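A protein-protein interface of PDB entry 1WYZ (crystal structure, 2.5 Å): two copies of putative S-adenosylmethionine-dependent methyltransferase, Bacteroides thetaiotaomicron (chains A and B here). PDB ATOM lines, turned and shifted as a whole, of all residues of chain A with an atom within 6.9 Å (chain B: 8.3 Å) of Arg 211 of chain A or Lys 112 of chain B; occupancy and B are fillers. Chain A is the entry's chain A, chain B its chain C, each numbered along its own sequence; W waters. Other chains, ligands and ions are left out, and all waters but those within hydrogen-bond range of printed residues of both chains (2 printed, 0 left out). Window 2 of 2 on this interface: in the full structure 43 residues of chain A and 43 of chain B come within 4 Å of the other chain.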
ATOM      1  N   SER A 131       9.830 -21.785   4.883  1.00  0.00           N
ATOM      2  CA  SER A 131       8.758 -21.818   3.894  1.00  0.00           C
ATOM      3  C   SER A 131       8.826 -23.081   3.066  1.00  0.00           C
ATOM      4  O   SER A 131       7.801 -23.585   2.614  1.00  0.00           O
ATOM      5  CB  SER A 131       8.817 -20.598   2.963  1.00  0.00           C
ATOM      6  OG  SER A 131       9.952 -20.628   2.108  1.00  0.00           O
ATOM      7  N   PHE A 133      10.371 -23.120   0.327  1.00  0.00           N
ATOM      8  CA  PHE A 133      10.475 -22.629  -1.035  1.00  0.00           C
ATOM      9  C   PHE A 133      11.928 -22.711  -1.488  1.00  0.00           C
ATOM     10  O   PHE A 133      12.819 -23.060  -0.702  1.00  0.00           O
ATOM     11  CB  PHE A 133      10.007 -21.178  -1.124  1.00  0.00           C
ATOM     12  CG  PHE A 133       8.534 -20.990  -0.855  1.00  0.00           C
ATOM     13  CD1 PHE A 133       7.628 -22.014  -1.127  1.00  0.00           C
ATOM     14  CD2 PHE A 133       8.044 -19.760  -0.401  1.00  0.00           C
ATOM     15  CE1 PHE A 133       6.249 -21.813  -0.961  1.00  0.00           C
ATOM     16  CE2 PHE A 133       6.672 -19.548  -0.231  1.00  0.00           C
ATOM     17  CZ  PHE A 133       5.769 -20.577  -0.511  1.00  0.00           C
ATOM     18  N   GLN A 192      -3.263 -21.173  -7.440  1.00  0.00           N
ATOM     19  CA  GLN A 192      -2.293 -22.226  -7.137  1.00  0.00           C
ATOM     20  C   GLN A 192      -0.922 -21.739  -6.672  1.00  0.00           C
ATOM     21  O   GLN A 192      -0.127 -22.517  -6.136  1.00  0.00           O
ATOM     22  CB  GLN A 192      -2.146 -23.171  -8.333  1.00  0.00           C
ATOM     23  CG  GLN A 192      -3.389 -24.045  -8.567  1.00  0.00           C
ATOM     24  CD  GLN A 192      -3.758 -24.876  -7.340  1.00  0.00           C
ATOM     25  OE1 GLN A 192      -4.760 -25.600  -7.338  1.00  0.00           O
ATOM     26  NE2 GLN A 192      -2.948 -24.779  -6.291  1.00  0.00           N
ATOM     27  N   THR A 193      -0.640 -20.454  -6.874  1.00  0.00           N
ATOM     28  CA  THR A 193       0.630 -19.894  -6.436  1.00  0.00           C
ATOM     29  C   THR A 193       0.659 -20.106  -4.921  1.00  0.00           C
ATOM     30  O   THR A 193      -0.396 -20.096  -4.273  1.00  0.00           O
ATOM     31  CB  THR A 193       0.706 -18.378  -6.738  1.00  0.00           C
ATOM     32  OG1 THR A 193       0.637 -18.157  -8.155  1.00  0.00           O
ATOM     33  CG2 THR A 193       1.994 -17.788  -6.199  1.00  0.00           C
ATOM     34  N   LYS A 194       1.850 -20.323  -4.358  1.00  0.00           N
ATOM     35  CA  LYS A 194       1.986 -20.524  -2.913  1.00  0.00           C
ATOM     36  C   LYS A 194       2.429 -19.251  -2.227  1.00  0.00           C
ATOM     37  O   LYS A 194       3.287 -18.516  -2.737  1.00  0.00           O
ATOM     38  CB  LYS A 194       2.997 -21.634  -2.585  1.00  0.00           C
ATOM     39  CG  LYS A 194       2.486 -23.052  -2.834  1.00  0.00           C
ATOM     40  CD  LYS A 194       3.363 -24.116  -2.160  1.00  0.00           C
ATOM     41  CE  LYS A 194       2.715 -25.492  -2.256  1.00  0.00           C
ATOM     42  NZ  LYS A 194       3.370 -26.511  -1.381  1.00  0.00           N
ATOM     43  N   LEU A 195       1.845 -19.006  -1.060  1.00  0.00           N
ATOM     44  CA  LEU A 195       2.166 -17.838  -0.261  1.00  0.00           C
ATOM     45  C   LEU A 195       2.550 -18.261   1.153  1.00  0.00           C
ATOM     46  O   LEU A 195       1.797 -18.980   1.806  1.00  0.00           O
ATOM     47  CB  LEU A 195       0.959 -16.902  -0.192  1.00  0.00           C
ATOM     48  CG  LEU A 195       1.047 -15.928   0.986  1.00  0.00           C
ATOM     49  CD1 LEU A 195       2.253 -15.037   0.789  1.00  0.00           C
ATOM     50  CD2 LEU A 195      -0.212 -15.089   1.097  1.00  0.00           C
ATOM     51  N   CYS A 196       3.715 -17.816   1.627  1.00  0.00           N
ATOM     52  CA  CYS A 196       4.161 -18.130   2.978  1.00  0.00           C
ATOM     53  C   CYS A 196       4.131 -16.864   3.833  1.00  0.00           C
ATOM     54  O   CYS A 196       4.729 -15.848   3.473  1.00  0.00           O
ATOM     55  CB  CYS A 196       5.585 -18.693   2.961  1.00  0.00           C
ATOM     56  SG  CYS A 196       6.333 -18.938   4.623  1.00  0.00           S
ATOM     57  N   ILE A 197       3.432 -16.924   4.959  1.00  0.00           N
ATOM     58  CA  ILE A 197       3.361 -15.792   5.860  1.00  0.00           C
ATOM     59  C   ILE A 197       4.292 -16.104   7.010  1.00  0.00           C
ATOM     60  O   ILE A 197       4.198 -17.172   7.607  1.00  0.00           O
ATOM     61  CB  ILE A 197       1.926 -15.596   6.395  1.00  0.00           C
ATOM     62  CG1 ILE A 197       1.031 -15.042   5.282  1.00  0.00           C
ATOM     63  CG2 ILE A 197       1.944 -14.678   7.618  1.00  0.00           C
ATOM     64  CD1 ILE A 197      -0.467 -15.105   5.570  1.00  0.00           C
ATOM     65  N   PHE A 207       4.958 -17.321  13.814  1.00  0.00           N
ATOM     66  CA  PHE A 207       3.981 -17.949  12.953  1.00  0.00           C
ATOM     67  C   PHE A 207       4.640 -17.995  11.581  1.00  0.00           C
ATOM     68  O   PHE A 207       4.998 -16.954  11.039  1.00  0.00           O
ATOM     69  CB  PHE A 207       2.705 -17.107  12.884  1.00  0.00           C
ATOM     70  CG  PHE A 207       1.662 -17.654  11.940  1.00  0.00           C
ATOM     71  CD1 PHE A 207       0.813 -18.691  12.336  1.00  0.00           C
ATOM     72  CD2 PHE A 207       1.542 -17.148  10.650  1.00  0.00           C
ATOM     73  CE1 PHE A 207      -0.157 -19.217  11.458  1.00  0.00           C
ATOM     74  CE2 PHE A 207       0.582 -17.660   9.755  1.00  0.00           C
ATOM     75  CZ  PHE A 207      -0.263 -18.697  10.166  1.00  0.00           C
ATOM     76  N   GLN A 209       3.881 -20.339   8.213  1.00  0.00           N
ATOM     77  CA  GLN A 209       3.144 -21.399   7.564  1.00  0.00           C
ATOM     78  C   GLN A 209       3.044 -21.110   6.077  1.00  0.00           C
ATOM     79  O   GLN A 209       2.880 -19.961   5.668  1.00  0.00           O
ATOM     80  CB  GLN A 209       1.756 -21.444   8.201  1.00  0.00           C
ATOM     81  CG  GLN A 209       0.886 -22.603   7.813  1.00  0.00           C
ATOM     82  CD  GLN A 209      -0.399 -22.613   8.620  1.00  0.00           C
ATOM     83  OE1 GLN A 209      -1.175 -21.656   8.583  1.00  0.00           O
ATOM     84  NE2 GLN A 209      -0.624 -23.692   9.361  1.00  0.00           N
ATOM     85  N   THR A 210       3.161 -22.156   5.271  1.00  0.00           N
ATOM     86  CA  THR A 210       3.060 -22.018   3.827  1.00  0.00           C
ATOM     87  C   THR A 210       1.718 -22.562   3.392  1.00  0.00           C
ATOM     88  O   THR A 210       1.212 -23.527   3.955  1.00  0.00           O
ATOM     89  CB  THR A 210       4.161 -22.786   3.098  1.00  0.00           C
ATOM     90  OG1 THR A 210       5.410 -22.125   3.314  1.00  0.00           O
ATOM     91  CG2 THR A 210       3.879 -22.839   1.610  1.00  0.00           C
ATOM     92  N   ARG A 211       1.150 -21.955   2.365  1.00  0.00           N
ATOM     93  CA  ARG A 211      -0.145 -22.388   1.906  1.00  0.00           C
ATOM     94  C   ARG A 211      -0.537 -21.644   0.643  1.00  0.00           C
ATOM     95  O   ARG A 211      -0.231 -20.463   0.482  1.00  0.00           O
ATOM     96  CB  ARG A 211      -1.138 -22.128   3.028  1.00  0.00           C
ATOM     97  CG  ARG A 211      -2.568 -22.092   2.641  1.00  0.00           C
ATOM     98  CD  ARG A 211      -3.340 -21.579   3.827  1.00  0.00           C
ATOM     99  NE  ARG A 211      -3.138 -22.428   4.989  1.00  0.00           N
ATOM    100  CZ  ARG A 211      -3.596 -22.145   6.200  1.00  0.00           C
ATOM    101  NH1 ARG A 211      -4.278 -21.024   6.400  1.00  0.00           N
ATOM    102  NH2 ARG A 211      -3.377 -22.982   7.207  1.00  0.00           N
ATOM    103  N   THR A 212      -1.213 -22.353  -0.252  1.00  0.00           N
ATOM    104  CA  THR A 212      -1.653 -21.785  -1.518  1.00  0.00           C
ATOM    105  C   THR A 212      -2.626 -20.613  -1.315  1.00  0.00           C
ATOM    106  O   THR A 212      -3.325 -20.535  -0.294  1.00  0.00           O
ATOM    107  CB  THR A 212      -2.319 -22.875  -2.389  1.00  0.00           C
ATOM    108  OG1 THR A 212      -2.478 -22.385  -3.721  1.00  0.00           O
ATOM    109  CG2 THR A 212      -3.688 -23.255  -1.832  1.00  0.00           C
ATOM    110  N   VAL A 213      -2.674 -19.700  -2.285  1.00  0.00           N
ATOM    111  CA  VAL A 213      -3.569 -18.547  -2.189  1.00  0.00           C
ATOM    112  C   VAL A 213      -5.034 -18.970  -2.031  1.00  0.00           C
ATOM    113  O   VAL A 213      -5.791 -18.337  -1.291  1.00  0.00           O
ATOM    114  CB  VAL A 213      -3.420 -17.634  -3.420  1.00  0.00           C
ATOM    115  CG1 VAL A 213      -4.507 -16.566  -3.431  1.00  0.00           C
ATOM    116  CG2 VAL A 213      -2.061 -16.976  -3.391  1.00  0.00           C
ATOM    117  N   LYS A 214      -5.421 -20.037  -2.727  1.00  0.00           N
ATOM    118  CA  LYS A 214      -6.780 -20.556  -2.649  1.00  0.00           C
ATOM    119  C   LYS A 214      -7.094 -20.994  -1.223  1.00  0.00           C
ATOM    120  O   LYS A 214      -8.175 -20.724  -0.713  1.00  0.00           O
ATOM    121  CB  LYS A 214      -6.954 -21.753  -3.588  1.00  0.00           C
ATOM    122  CG  LYS A 214      -8.355 -22.361  -3.567  1.00  0.00           C
ATOM    123  CD  LYS A 214      -8.392 -23.734  -4.222  1.00  0.00           C
ATOM    124  CE  LYS A 214      -9.810 -24.278  -4.281  1.00  0.00           C
ATOM    125  NZ  LYS A 214     -10.700 -23.452  -5.160  1.00  0.00           N
ATOM    126  N   ASP A 215      -6.145 -21.674  -0.584  1.00  0.00           N
ATOM    127  CA  ASP A 215      -6.345 -22.152   0.785  1.00  0.00           C
ATOM    128  C   ASP A 215      -6.124 -21.101   1.865  1.00  0.00           C
ATOM    129  O   ASP A 215      -6.396 -21.357   3.035  1.00  0.00           O
ATOM    130  CB  ASP A 215      -5.472 -23.387   1.068  1.00  0.00           C
ATOM    131  CG  ASP A 215      -6.015 -24.655   0.406  1.00  0.00           C
ATOM    132  OD1 ASP A 215      -7.180 -25.025   0.689  1.00  0.00           O
ATOM    133  OD2 ASP A 215      -5.278 -25.280  -0.393  1.00  0.00           O
ATOM    134  N   TRP A 216      -5.633 -19.927   1.483  1.00  0.00           N
ATOM    135  CA  TRP A 216      -5.428 -18.863   2.454  1.00  0.00           C
ATOM    136  C   TRP A 216      -6.745 -18.112   2.644  1.00  0.00           C
ATOM    137  O   TRP A 216      -7.036 -17.613   3.733  1.00  0.00           O
ATOM    138  CB  TRP A 216      -4.334 -17.894   1.988  1.00  0.00           C
ATOM    139  CG  TRP A 216      -2.957 -18.191   2.551  1.00  0.00           C
ATOM    140  CD1 TRP A 216      -1.815 -18.424   1.845  1.00  0.00           C
ATOM    141  CD2 TRP A 216      -2.587 -18.249   3.939  1.00  0.00           C
ATOM    142  NE1 TRP A 216      -0.754 -18.619   2.703  1.00  0.00           N
ATOM    143  CE2 TRP A 216      -1.201 -18.518   3.994  1.00  0.00           C
ATOM    144  CE3 TRP A 216      -3.292 -18.096   5.141  1.00  0.00           C
ATOM    145  CZ2 TRP A 216      -0.503 -18.640   5.203  1.00  0.00           C
ATOM    146  CZ3 TRP A 216      -2.600 -18.214   6.348  1.00  0.00           C
ATOM    147  CH2 TRP A 216      -1.216 -18.484   6.368  1.00  0.00           C
ATOM    148  N   LYS A 217      -7.542 -18.053   1.578  1.00  0.00           N
ATOM    149  CA  LYS A 217      -8.829 -17.364   1.603  1.00  0.00           C
ATOM    150  C   LYS A 217      -9.466 -17.510   2.968  1.00  0.00           C
ATOM    151  O   LYS A 217      -9.721 -16.522   3.657  1.00  0.00           O
ATOM    152  CB  LYS A 217      -9.754 -17.938   0.531  1.00  0.00           C
ATOM    153  CG  LYS A 217      -9.227 -17.759  -0.892  1.00  0.00           C
ATOM    154  CD  LYS A 217      -9.114 -16.279  -1.267  1.00  0.00           C
ATOM    155  CE  LYS A 217      -8.496 -16.090  -2.647  1.00  0.00           C
ATOM    156  NZ  LYS A 217      -9.293 -16.722  -3.733  1.00  0.00           N
ATOM    157  N   GLY A 218      -9.715 -18.749   3.362  1.00  0.00           N
ATOM    158  CA  GLY A 218     -10.296 -18.980   4.665  1.00  0.00           C
ATOM    159  C   GLY A 218      -9.149 -19.042   5.645  1.00  0.00           C
ATOM    160  O   GLY A 218      -8.049 -19.456   5.281  1.00  0.00           O
ATOM    161  N   HIS A 219      -9.384 -18.625   6.881  1.00  0.00           N
ATOM    162  CA  HIS A 219      -8.335 -18.664   7.890  1.00  0.00           C
ATOM    163  C   HIS A 219      -7.161 -17.719   7.633  1.00  0.00           C
ATOM    164  O   HIS A 219      -6.089 -18.143   7.195  1.00  0.00           O
ATOM    165  CB  HIS A 219      -7.801 -20.096   8.050  1.00  0.00           C
ATOM    166  CG  HIS A 219      -8.628 -20.951   8.960  1.00  0.00           C
ATOM    167  ND1 HIS A 219      -9.942 -21.273   8.692  1.00  0.00           N
ATOM    168  CD2 HIS A 219      -8.334 -21.535  10.146  1.00  0.00           C
ATOM    169  CE1 HIS A 219     -10.421 -22.015   9.674  1.00  0.00           C
ATOM    170  NE2 HIS A 219      -9.465 -22.189  10.570  1.00  0.00           N
ATOM    171  N   ILE A 220      -7.373 -16.436   7.911  1.00  0.00           N
ATOM    172  CA  ILE A 220      -6.337 -15.423   7.768  1.00  0.00           C
ATOM    173  C   ILE A 220      -6.011 -14.961   9.197  1.00  0.00           C
ATOM    174  O   ILE A 220      -6.876 -14.436   9.904  1.00  0.00           O
ATOM    175  CB  ILE A 220      -6.841 -14.233   6.929  1.00  0.00           C
ATOM    176  CG1 ILE A 220      -5.742 -13.173   6.812  1.00  0.00           C
ATOM    177  CG2 ILE A 220      -8.103 -13.647   7.556  1.00  0.00           C
ATOM    178  CD1 ILE A 220      -4.599 -13.535   5.867  1.00  0.00           C
ATOM    179  N   PRO A 221      -4.761 -15.155   9.643  1.00  0.00           N
ATOM    180  CA  PRO A 221      -4.338 -14.764  10.992  1.00  0.00           C
ATOM    181  C   PRO A 221      -4.297 -13.261  11.250  1.00  0.00           C
ATOM    182  O   PRO A 221      -5.263 -12.556  10.985  1.00  0.00           O
ATOM    183  CB  PRO A 221      -2.965 -15.417  11.113  1.00  0.00           C
ATOM    184  CG  PRO A 221      -2.435 -15.296   9.727  1.00  0.00           C
ATOM    185  CD  PRO A 221      -3.625 -15.692   8.874  1.00  0.00           C
ATOM    186  N   LEU A 231       6.366 -14.553   1.299  1.00  0.00           N
ATOM    187  CA  LEU A 231       7.092 -15.277   0.262  1.00  0.00           C
ATOM    188  C   LEU A 231       6.149 -15.937  -0.736  1.00  0.00           C
ATOM    189  O   LEU A 231       5.239 -16.661  -0.349  1.00  0.00           O
ATOM    190  CB  LEU A 231       7.987 -16.356   0.870  1.00  0.00           C
ATOM    191  CG  LEU A 231       9.048 -15.937   1.885  1.00  0.00           C
ATOM    192  CD1 LEU A 231       8.371 -15.674   3.234  1.00  0.00           C
ATOM    193  CD2 LEU A 231      10.114 -17.043   2.018  1.00  0.00           C
ATOM    194  N   LEU B  80       7.091 -36.434  14.474  1.00  0.00           N
ATOM    195  CA  LEU B  80       6.740 -35.022  14.689  1.00  0.00           C
ATOM    196  C   LEU B  80       5.216 -34.893  14.772  1.00  0.00           C
ATOM    197  O   LEU B  80       4.686 -34.260  15.687  1.00  0.00           O
ATOM    198  CB  LEU B  80       7.294 -34.158  13.548  1.00  0.00           C
ATOM    199  CG  LEU B  80       6.858 -32.689  13.444  1.00  0.00           C
ATOM    200  CD1 LEU B  80       6.983 -31.977  14.792  1.00  0.00           C
ATOM    201  CD2 LEU B  80       7.713 -31.992  12.381  1.00  0.00           C
ATOM    202  N   ALA B  81       4.524 -35.510  13.820  1.00  0.00           N
ATOM    203  CA  ALA B  81       3.068 -35.488  13.809  1.00  0.00           C
ATOM    204  C   ALA B  81       2.539 -36.008  15.155  1.00  0.00           C
ATOM    205  O   ALA B  81       1.527 -35.521  15.670  1.00  0.00           O
ATOM    206  CB  ALA B  81       2.527 -36.347  12.656  1.00  0.00           C
ATOM    207  N   VAL B 105      10.748 -29.704   4.585  1.00  0.00           N
ATOM    208  CA  VAL B 105      10.080 -28.581   5.231  1.00  0.00           C
ATOM    209  C   VAL B 105       8.761 -28.360   4.487  1.00  0.00           C
ATOM    210  O   VAL B 105       7.705 -28.174   5.098  1.00  0.00           O
ATOM    211  CB  VAL B 105      10.953 -27.307   5.163  1.00  0.00           C
ATOM    212  CG1 VAL B 105      10.234 -26.132   5.801  1.00  0.00           C
ATOM    213  CG2 VAL B 105      12.262 -27.551   5.870  1.00  0.00           C
ATOM    214  N   ALA B 106       8.831 -28.411   3.160  1.00  0.00           N
ATOM    215  CA  ALA B 106       7.658 -28.216   2.326  1.00  0.00           C
ATOM    216  C   ALA B 106       6.525 -29.168   2.694  1.00  0.00           C
ATOM    217  O   ALA B 106       5.392 -28.738   2.923  1.00  0.00           O
ATOM    218  CB  ALA B 106       8.020 -28.389   0.856  1.00  0.00           C
ATOM    219  N   ILE B 107       6.819 -30.462   2.750  1.00  0.00           N
ATOM    220  CA  ILE B 107       5.784 -31.430   3.080  1.00  0.00           C
ATOM    221  C   ILE B 107       5.289 -31.269   4.516  1.00  0.00           C
ATOM    222  O   ILE B 107       4.105 -31.467   4.796  1.00  0.00           O
ATOM    223  CB  ILE B 107       6.272 -32.872   2.816  1.00  0.00           C
ATOM    224  CG1 ILE B 107       6.513 -33.044   1.308  1.00  0.00           C
ATOM    225  CG2 ILE B 107       5.244 -33.876   3.311  1.00  0.00           C
ATOM    226  CD1 ILE B 107       7.316 -34.284   0.922  1.00  0.00           C
ATOM    227  N   ALA B 108       6.188 -30.895   5.421  1.00  0.00           N
ATOM    228  CA  ALA B 108       5.799 -30.687   6.806  1.00  0.00           C
ATOM    229  C   ALA B 108       4.767 -29.558   6.826  1.00  0.00           C
ATOM    230  O   ALA B 108       3.804 -29.600   7.601  1.00  0.00           O
ATOM    231  CB  ALA B 108       7.008 -30.314   7.639  1.00  0.00           C
ATOM    232  N   GLN B 109       4.981 -28.560   5.960  1.00  0.00           N
ATOM    233  CA  GLN B 109       4.093 -27.395   5.813  1.00  0.00           C
ATOM    234  C   GLN B 109       2.724 -27.817   5.276  1.00  0.00           C
ATOM    235  O   GLN B 109       1.686 -27.360   5.749  1.00  0.00           O
ATOM    236  CB  GLN B 109       4.711 -26.369   4.843  1.00  0.00           C
ATOM    237  CG  GLN B 109       5.767 -25.448   5.452  1.00  0.00           C
ATOM    238  CD  GLN B 109       5.188 -24.433   6.448  1.00  0.00           C
ATOM    239  OE1 GLN B 109       5.925 -23.722   7.143  1.00  0.00           O
ATOM    240  NE2 GLN B 109       3.869 -24.361   6.510  1.00  0.00           N
ATOM    241  N   ARG B 110       2.746 -28.683   4.272  1.00  0.00           N
ATOM    242  CA  ARG B 110       1.532 -29.180   3.653  1.00  0.00           C
ATOM    243  C   ARG B 110       0.727 -29.936   4.705  1.00  0.00           C
ATOM    244  O   ARG B 110      -0.498 -29.863   4.727  1.00  0.00           O
ATOM    245  CB  ARG B 110       1.889 -30.094   2.469  1.00  0.00           C
ATOM    246  CG  ARG B 110       0.710 -30.731   1.747  1.00  0.00           C
ATOM    247  CD  ARG B 110       1.034 -32.164   1.308  1.00  0.00           C
ATOM    248  NE  ARG B 110       1.308 -32.307  -0.131  1.00  0.00           N
ATOM    249  CZ  ARG B 110       2.472 -32.047  -0.728  1.00  0.00           C
ATOM    250  NH1 ARG B 110       3.508 -31.622  -0.023  1.00  0.00           N
ATOM    251  NH2 ARG B 110       2.598 -32.216  -2.039  1.00  0.00           N
ATOM    252  N   GLN B 111       1.413 -30.661   5.581  1.00  0.00           N
ATOM    253  CA  GLN B 111       0.726 -31.410   6.632  1.00  0.00           C
ATOM    254  C   GLN B 111       0.531 -30.503   7.840  1.00  0.00           C
ATOM    255  O   GLN B 111       0.376 -30.969   8.960  1.00  0.00           O
ATOM    256  CB  GLN B 111       1.531 -32.661   7.014  1.00  0.00           C
ATOM    257  CG  GLN B 111       1.851 -33.593   5.818  1.00  0.00           C
ATOM    258  CD  GLN B 111       2.610 -34.872   6.207  1.00  0.00           C
ATOM    259  OE1 GLN B 111       2.961 -35.683   5.344  1.00  0.00           O
ATOM    260  NE2 GLN B 111       2.863 -35.052   7.500  1.00  0.00           N
ATOM    261  N   LYS B 112       0.536 -29.199   7.581  1.00  0.00           N
ATOM    262  CA  LYS B 112       0.354 -28.167   8.600  1.00  0.00           C
ATOM    263  C   LYS B 112       1.087 -28.396   9.918  1.00  0.00           C
ATOM    264  O   LYS B 112       0.540 -28.132  10.990  1.00  0.00           O
ATOM    265  CB  LYS B 112      -1.139 -27.955   8.867  1.00  0.00           C
ATOM    266  CG  LYS B 112      -1.921 -27.492   7.643  1.00  0.00           C
ATOM    267  CD  LYS B 112      -3.418 -27.416   7.932  1.00  0.00           C
ATOM    268  CE  LYS B 112      -4.199 -26.794   6.774  1.00  0.00           C
ATOM    269  NZ  LYS B 112      -5.655 -26.689   7.080  1.00  0.00           N
ATOM    270  N   LEU B 113       2.328 -28.876   9.828  1.00  0.00           N
ATOM    271  CA  LEU B 113       3.163 -29.116  11.004  1.00  0.00           C
ATOM    272  C   LEU B 113       3.965 -27.848  11.309  1.00  0.00           C
ATOM    273  O   LEU B 113       4.212 -27.027  10.427  1.00  0.00           O
ATOM    274  CB  LEU B 113       4.119 -30.301  10.767  1.00  0.00           C
ATOM    275  CG  LEU B 113       3.451 -31.653  10.447  1.00  0.00           C
ATOM    276  CD1 LEU B 113       4.494 -32.676  10.027  1.00  0.00           C
ATOM    277  CD2 LEU B 113       2.672 -32.147  11.651  1.00  0.00           C
ATOM    278  N   LYS B 114       4.356 -27.692  12.567  1.00  0.00           N
ATOM    279  CA  LYS B 114       5.111 -26.531  13.019  1.00  0.00           C
ATOM    280  C   LYS B 114       6.584 -26.603  12.619  1.00  0.00           C
ATOM    281  O   LYS B 114       7.301 -27.529  13.024  1.00  0.00           O
ATOM    282  CB  LYS B 114       5.019 -26.434  14.533  1.00  0.00           C
ATOM    283  CG  LYS B 114       5.725 -25.245  15.125  1.00  0.00           C
ATOM    284  CD  LYS B 114       5.004 -23.976  14.769  1.00  0.00           C
ATOM    285  CE  LYS B 114       5.535 -22.844  15.598  1.00  0.00           C
ATOM    286  NZ  LYS B 114       5.410 -23.185  17.036  1.00  0.00           N
ATOM    287  N   VAL B 115       7.031 -25.627  11.831  1.00  0.00           N
ATOM    288  CA  VAL B 115       8.420 -25.579  11.396  1.00  0.00           C
ATOM    289  C   VAL B 115       9.014 -24.382  12.101  1.00  0.00           C
ATOM    290  O   VAL B 115       8.402 -23.317  12.158  1.00  0.00           O
ATOM    291  CB  VAL B 115       8.563 -25.345   9.873  1.00  0.00           C
ATOM    292  CG1 VAL B 115       9.984 -25.662   9.437  1.00  0.00           C
ATOM    293  CG2 VAL B 115       7.554 -26.182   9.111  1.00  0.00           C
HETATM  294  O   HOH W   1       1.817 -26.070   2.192  1.00  0.00           O
HETATM  295  O   HOH W   2       4.420 -26.736   1.051  1.00  0.00           O
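NE2 of Gln 109 of chain B lies close to N of Thr 210 of chain A.
OG of Ser 131 of chain A lies within hydrogen-bond range of N of Phe 133 of chain A, 3.1 Å away. The backbone NH of Leu 195 of chain A is in hydrogen-bond range of the backbone carbonyl oxygen of Arg 211 of chain A. O of Gln 209 of chain A lies close to SG of Cys 196 of chain A. O of Gln 209 of chain A is in hydrogen-bond range of N of Ile 197 of chain A (3.2 Å). OE1 of Gln 209 of chain A is in hydrogen-bond range of NH2 of Arg 211 of chain A. O of His 219 of chain A lies within hydrogen-bond range of NH1 of Arg 211 of chain A, 3.5 Å away.
Ser 131 of chain A touches Gln 109 of chain B (O to CG, 3.96 Å). NE2 of Gln 109 of chain B touches CA of Gln 209 of chain A (3.2 Å). NH2 of Arg 211 of chain A touches CE of Lys 112 of chain B, at 3.9 Å.
Of the printed residues of chain B, Ser 131 of chain A touches Gln 109 (3.96 Å). Printed residues of chain B within 4 Å of Gln 209 of chain A: Gln 109. Printed residues of chain B within 4 Å of Thr 210 of chain A: Gln 109 (2.6 Å). Arg 211 of chain A touches just one residue of chain B: Lys 112. Lys 217 of chain A touches none of the printed residues of chain B. Ile 107 of chain B touches none of the printed residues of chain A. Of the printed residues of chain A, Gln 109 of chain B touches Ser 131, Gln 209 and Thr 210. Lys 112 of chain B touches just one residue of chain A: Arg 211. The nearest residue of chain B that does not touch Arg 211 of chain A is Gln 109 of chain B (5.5 Å). The nearest residue of chain A that does not touch Lys 112 of chain B is Gln 209 of chain A (4.3 Å). The nearest printed residue of chain B that does not touch Thr 210 of chain A is Arg 110 of chain B (5.4 Å).
Along chain B the printed residues that touch a printed residue of chain A span positions 109 to 112. Among the printed residues, no Asp or Glu carboxylate lies within 4 Å of a Lys or Arg side-chain nitrogen of the other chain.
No position is printed for both chains. Of the 4 pairs that touch across the chains among the printed residues, none has its exchanged pair printed and touching as well.
Water W2 lies within hydrogen-bond range of NZ of Lys 194 of chain A (2.7 Å) and O of Ala 106 of chain B (2.9 Å). Water W1 bridges the backbone carbonyl oxygen (O) of Thr 210 of chain A and the backbone NH (N) of Arg 110 of chain B.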
